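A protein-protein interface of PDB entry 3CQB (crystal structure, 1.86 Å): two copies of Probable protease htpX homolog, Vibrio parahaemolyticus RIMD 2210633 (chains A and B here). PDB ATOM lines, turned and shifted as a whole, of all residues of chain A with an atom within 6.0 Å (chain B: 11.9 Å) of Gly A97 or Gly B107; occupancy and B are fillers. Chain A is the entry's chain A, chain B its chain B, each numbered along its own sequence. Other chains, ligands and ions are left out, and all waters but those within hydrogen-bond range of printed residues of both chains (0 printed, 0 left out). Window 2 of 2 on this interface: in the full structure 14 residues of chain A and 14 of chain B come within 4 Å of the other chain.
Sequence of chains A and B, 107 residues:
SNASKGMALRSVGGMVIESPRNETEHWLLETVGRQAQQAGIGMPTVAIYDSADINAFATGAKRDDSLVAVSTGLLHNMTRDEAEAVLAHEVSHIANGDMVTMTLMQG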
ATOM      1  N   GLY A  60     -11.035  22.847 -22.073  1.00  0.00           N
ATOM      2  CA  GLY A  60     -10.556  22.654 -23.455  1.00  0.00           C
ATOM      3  C   GLY A  60      -9.435  23.616 -23.805  1.00  0.00           C
ATOM      4  O   GLY A  60      -9.196  23.901 -24.993  1.00  0.00           O
ATOM      5  N   ALA A  61      -8.729  24.113 -22.783  1.00  0.00           N
ATOM      6  CA  ALA A  61      -7.679  25.131 -22.997  1.00  0.00           C
ATOM      7  C   ALA A  61      -6.484  24.637 -23.834  1.00  0.00           C
ATOM      8  O   ALA A  61      -5.820  25.433 -24.506  1.00  0.00           O
ATOM      9  CB  ALA A  61      -7.202  25.712 -21.666  1.00  0.00           C
ATOM     10  N   SER A  92     -19.908  22.184 -25.046  1.00  0.00           N
ATOM     11  CA  SER A  92     -19.970  23.396 -25.887  1.00  0.00           C
ATOM     12  C   SER A  92     -18.889  24.414 -25.497  1.00  0.00           C
ATOM     13  O   SER A  92     -18.364  25.122 -26.352  1.00  0.00           O
ATOM     14  CB  SER A  92     -21.352  24.063 -25.836  1.00  0.00           C
ATOM     15  OG  SER A  92     -21.538  24.872 -24.678  1.00  0.00           O
ATOM     16  N   HIS A  93     -18.591  24.518 -24.206  1.00  0.00           N
ATOM     17  CA  HIS A  93     -17.515  25.381 -23.729  1.00  0.00           C
ATOM     18  C   HIS A  93     -16.139  24.888 -24.109  1.00  0.00           C
ATOM     19  O   HIS A  93     -15.284  25.687 -24.534  1.00  0.00           O
ATOM     20  CB  HIS A  93     -17.640  25.600 -22.202  1.00  0.00           C
ATOM     21  CG  HIS A  93     -18.843  26.403 -21.843  1.00  0.00           C
ATOM     22  ND1 HIS A  93     -19.031  27.682 -22.324  1.00  0.00           N
ATOM     23  CD2 HIS A  93     -19.947  26.099 -21.118  1.00  0.00           C
ATOM     24  CE1 HIS A  93     -20.202  28.132 -21.908  1.00  0.00           C
ATOM     25  NE2 HIS A  93     -20.774  27.193 -21.165  1.00  0.00           N
ATOM     26  N   ILE A  94     -15.917  23.585 -23.971  1.00  0.00           N
ATOM     27  CA  ILE A  94     -14.650  22.986 -24.377  1.00  0.00           C
ATOM     28  C   ILE A  94     -14.447  23.293 -25.838  1.00  0.00           C
ATOM     29  O   ILE A  94     -13.316  23.623 -26.267  1.00  0.00           O
ATOM     30  CB  ILE A  94     -14.644  21.444 -24.262  1.00  0.00           C
ATOM     31  CG1 ILE A  94     -14.690  20.978 -22.813  1.00  0.00           C
ATOM     32  CG2 ILE A  94     -13.388  20.888 -24.939  1.00  0.00           C
ATOM     33  CD1 ILE A  94     -14.854  19.418 -22.692  1.00  0.00           C
ATOM     34  N   ALA A  95     -15.520  23.158 -26.621  1.00  0.00           N
ATOM     35  CA  ALA A  95     -15.393  23.337 -28.081  1.00  0.00           C
ATOM     36  C   ALA A  95     -14.957  24.764 -28.425  1.00  0.00           C
ATOM     37  O   ALA A  95     -14.288  24.991 -29.444  1.00  0.00           O
ATOM     38  CB  ALA A  95     -16.683  22.968 -28.794  1.00  0.00           C
ATOM     39  N   ASN A  96     -15.319  25.723 -27.577  1.00  0.00           N
ATOM     40  CA  ASN A  96     -14.837  27.096 -27.697  1.00  0.00           C
ATOM     41  C   ASN A  96     -13.421  27.342 -27.151  1.00  0.00           C
ATOM     42  O   ASN A  96     -12.947  28.476 -27.171  1.00  0.00           O
ATOM     43  CB  ASN A  96     -15.797  28.058 -27.011  1.00  0.00           C
ATOM     44  CG  ASN A  96     -17.133  28.137 -27.692  1.00  0.00           C
ATOM     45  OD1 ASN A  96     -17.246  27.850 -28.893  1.00  0.00           O
ATOM     46  ND2 ASN A  96     -18.160  28.583 -26.954  1.00  0.00           N
ATOM     47  N   GLY A  97     -12.740  26.298 -26.696  1.00  0.00           N
ATOM     48  CA  GLY A  97     -11.435  26.432 -26.044  1.00  0.00           C
ATOM     49  C   GLY A  97     -11.507  27.099 -24.670  1.00  0.00           C
ATOM     50  O   GLY A  97     -10.512  27.664 -24.177  1.00  0.00           O
ATOM     51  N   ASP A  98     -12.665  26.992 -24.022  1.00  0.00           N
ATOM     52  CA  ASP A  98     -12.860  27.598 -22.704  1.00  0.00           C
ATOM     53  C   ASP A  98     -12.880  26.547 -21.588  1.00  0.00           C
ATOM     54  O   ASP A  98     -12.742  25.334 -21.844  1.00  0.00           O
ATOM     55  CB  ASP A  98     -14.136  28.441 -22.684  1.00  0.00           C
ATOM     56  CG  ASP A  98     -14.050  29.669 -23.607  1.00  0.00           C
ATOM     57  OD1 ASP A  98     -12.916  30.137 -23.907  1.00  0.00           O
ATOM     58  OD2 ASP A  98     -15.128  30.152 -24.023  1.00  0.00           O
ATOM     59  N   MET A  99     -12.989  27.019 -20.346  1.00  0.00           N
ATOM     60  CA  MET A  99     -13.005  26.128 -19.180  1.00  0.00           C
ATOM     61  C   MET A  99     -14.290  26.437 -18.417  1.00  0.00           C
ATOM     62  O   MET A  99     -14.746  27.595 -18.400  1.00  0.00           O
ATOM     63  CB  MET A  99     -11.778  26.404 -18.288  1.00  0.00           C
ATOM     64  CG  MET A  99     -10.392  26.011 -18.906  1.00  0.00           C
ATOM     65  SD  MET A  99      -8.958  27.217 -18.386  1.00  0.00           S
ATOM     66  CE  MET A  99      -9.339  28.585 -19.707  1.00  0.00           C
ATOM     67  N   ILE B  54     -16.358  35.319 -14.200  1.00  0.00           N
ATOM     68  CA  ILE B  54     -17.439  35.169 -15.168  1.00  0.00           C
ATOM     69  C   ILE B  54     -18.385  34.112 -14.572  1.00  0.00           C
ATOM     70  O   ILE B  54     -18.097  32.918 -14.621  1.00  0.00           O
ATOM     71  CB  ILE B  54     -16.903  34.693 -16.534  1.00  0.00           C
ATOM     72  CG1 ILE B  54     -15.923  35.721 -17.130  1.00  0.00           C
ATOM     73  CG2 ILE B  54     -18.102  34.359 -17.485  1.00  0.00           C
ATOM     74  CD1 ILE B  54     -15.086  35.097 -18.333  1.00  0.00           C
ATOM     75  N   ASN B  77     -17.164  40.329 -20.024  1.00  0.00           N
ATOM     76  CA  ASN B  77     -16.327  39.439 -20.820  1.00  0.00           C
ATOM     77  C   ASN B  77     -17.042  38.582 -21.859  1.00  0.00           C
ATOM     78  O   ASN B  77     -16.408  38.121 -22.806  1.00  0.00           O
ATOM     79  CB  ASN B  77     -15.538  38.510 -19.885  1.00  0.00           C
ATOM     80  CG  ASN B  77     -14.464  39.248 -19.136  1.00  0.00           C
ATOM     81  OD1 ASN B  77     -13.479  39.654 -19.722  1.00  0.00           O
ATOM     82  ND2 ASN B  77     -14.669  39.463 -17.843  1.00  0.00           N
ATOM     83  N   MET B  78     -18.340  38.357 -21.676  1.00  0.00           N
ATOM     84  CA  MET B  78     -19.097  37.500 -22.593  1.00  0.00           C
ATOM     85  C   MET B  78     -19.784  38.309 -23.677  1.00  0.00           C
ATOM     86  O   MET B  78     -20.284  39.401 -23.403  1.00  0.00           O
ATOM     87  CB  MET B  78     -20.170  36.733 -21.822  1.00  0.00           C
ATOM     88  CG  MET B  78     -19.607  35.929 -20.695  1.00  0.00           C
ATOM     89  SD  MET B  78     -18.586  34.515 -21.482  1.00  0.00           S
ATOM     90  CE  MET B  78     -20.036  33.199 -21.570  1.00  0.00           C
ATOM     91  N   GLU B  82     -22.849  34.368 -26.346  1.00  0.00           N
ATOM     92  CA  GLU B  82     -22.256  33.486 -25.321  1.00  0.00           C
ATOM     93  C   GLU B  82     -23.046  33.500 -24.037  1.00  0.00           C
ATOM     94  O   GLU B  82     -23.327  32.449 -23.459  1.00  0.00           O
ATOM     95  CB  GLU B  82     -20.796  33.882 -25.023  1.00  0.00           C
ATOM     96  CG  GLU B  82     -19.861  33.676 -26.193  1.00  0.00           C
ATOM     97  CD  GLU B  82     -18.466  34.343 -26.025  1.00  0.00           C
ATOM     98  OE1 GLU B  82     -18.265  35.341 -25.249  1.00  0.00           O
ATOM     99  OE2 GLU B  82     -17.555  33.850 -26.727  1.00  0.00           O
ATOM    100  N   THR B 103     -19.267  28.833 -13.518  1.00  0.00           N
ATOM    101  CA  THR B 103     -18.196  29.804 -13.648  1.00  0.00           C
ATOM    102  C   THR B 103     -17.343  29.404 -14.838  1.00  0.00           C
ATOM    103  O   THR B 103     -17.075  28.198 -15.041  1.00  0.00           O
ATOM    104  CB  THR B 103     -17.360  29.886 -12.352  1.00  0.00           C
ATOM    105  OG1 THR B 103     -18.241  30.242 -11.266  1.00  0.00           O
ATOM    106  CG2 THR B 103     -16.252  30.954 -12.463  1.00  0.00           C
ATOM    107  N   LEU B 104     -16.943  30.404 -15.626  1.00  0.00           N
ATOM    108  CA  LEU B 104     -16.177  30.159 -16.847  1.00  0.00           C
ATOM    109  C   LEU B 104     -14.852  30.896 -16.850  1.00  0.00           C
ATOM    110  O   LEU B 104     -14.713  31.942 -16.202  1.00  0.00           O
ATOM    111  CB  LEU B 104     -16.959  30.616 -18.094  1.00  0.00           C
ATOM    112  CG  LEU B 104     -18.414  30.164 -18.302  1.00  0.00           C
ATOM    113  CD1 LEU B 104     -18.921  30.805 -19.565  1.00  0.00           C
ATOM    114  CD2 LEU B 104     -18.442  28.699 -18.519  1.00  0.00           C
ATOM    115  N   MET B 105     -13.898  30.363 -17.602  1.00  0.00           N
ATOM    116  CA  MET B 105     -12.667  31.095 -17.911  1.00  0.00           C
ATOM    117  C   MET B 105     -12.418  30.957 -19.393  1.00  0.00           C
ATOM    118  O   MET B 105     -12.533  29.864 -19.956  1.00  0.00           O
ATOM    119  CB  MET B 105     -11.470  30.527 -17.154  1.00  0.00           C
ATOM    120  CG  MET B 105     -11.492  30.871 -15.676  1.00  0.00           C
ATOM    121  SD  MET B 105     -10.074  29.982 -14.690  1.00  0.00           S
ATOM    122  CE  MET B 105      -8.697  29.809 -16.051  1.00  0.00           C
ATOM    123  N   GLN B 106     -12.028  32.052 -20.022  1.00  0.00           N
ATOM    124  CA  GLN B 106     -11.896  32.042 -21.468  1.00  0.00           C
ATOM    125  C   GLN B 106     -10.473  31.673 -21.825  1.00  0.00           C
ATOM    126  O   GLN B 106      -9.538  32.167 -21.200  1.00  0.00           O
ATOM    127  CB  GLN B 106     -12.311  33.408 -22.049  1.00  0.00           C
ATOM    128  CG  GLN B 106     -13.795  33.696 -21.756  1.00  0.00           C
ATOM    129  CD  GLN B 106     -14.261  35.111 -22.118  1.00  0.00           C
ATOM    130  OE1 GLN B 106     -13.548  36.118 -21.909  1.00  0.00           O
ATOM    131  NE2 GLN B 106     -15.483  35.190 -22.623  1.00  0.00           N
ATOM    132  N   GLY B 107     -10.305  30.793 -22.809  1.00  0.00           N
ATOM    133  CA  GLY B 107      -8.975  30.334 -23.219  1.00  0.00           C
ATOM    134  C   GLY B 107      -8.400  31.248 -24.293  1.00  0.00           C
ATOM    135  O   GLY B 107      -8.959  32.327 -24.539  1.00  0.00           O
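The backbone carbonyl oxygen (O) of Gly A97 lies close to the backbone NH (N) of Gly B107 (3.4 Å). The side-chain carboxylate (OD1) of Asp A98 lies within hydrogen-bond range of the backbone NH (N) of Gly B107, at 2.9 Å. The backbone NH (N) of Met A99 lies within hydrogen-bond range of the backbone carbonyl oxygen (O) of Met B105 (2.9 Å).
N of Gly A60 is in hydrogen-bond range of O of Asp A98, 3.0 Å away. N of Asp A98 is in hydrogen-bond range of O of His A93 (3.0 Å). O of Ile B54 sits at hydrogen-bond distance from N of Leu B104, 2.9 Å away. The side-chain amide nitrogen (NE2) of Gln B106 sits at hydrogen-bond distance from the backbone carbonyl oxygen (O) of Asn B77, at 3.1 Å. The side-chain sulfur of Met B78 is in hydrogen-bond range of the side-chain amide nitrogen of Gln B106 (3.4 Å).
Leu B104 touches His A93 (CD1 to CE1, 3.8 Å). Asp A98 touches Met B105 (CB to O, 3.5 Å). Gln B106 touches Asp A98 (CA to OD1, 3.3 Å). Leu B104 touches Met A99. Gln B106 touches Met A99 (O to CE, 3.9 Å). CE of Met A99 touches N of Gly B107, 3.9 Å away.
Gly B107 touches just these residues of chain A: Gly A97, Asp A98 and Met A99. Gly A60 touches none of the printed residues of chain B. No residue of chain B comes within 4 Å of Ala A61. No residue of chain B comes within 4 Å of Asn A96. Of chain B, only Leu B104, Met B105, Gln B106 and Gly B107 come within 4 Å of Met A99. Printed residues of chain A within 4 Å of Met B105: Asp A98 and Met A99. Of the printed residues of chain B, His A93 touches Leu B104 (3.8 Å). Printed residues of chain A within 4 Å of Gln B106: Asp A98 and Met A99. Met B78 touches none of the printed residues of chain A. Ser A92 touches none of the printed residues of chain B. The nearest printed residue of chain B that does not touch His A93 is Met B78 (5.1 Å).
Of the 9 printed residues of chain B, 4 touch a printed residue of chain A. Hydrophobic or aromatic side chains of chain B that line the printed part of chain A: Leu B104 and Met B105. Of the 10 printed residues of chain A, 4 touch a printed residue of chain B. Along chain A the printed residues that touch a printed residue of chain B span positions 93 to 99. Among the printed residues, 9 pairs touch across the chains. Among the printed residues, no Asp or Glu carboxylate lies within 4 Å of a Lys or Arg side-chain nitrogen of the other chain.
No position is printed for both chains.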
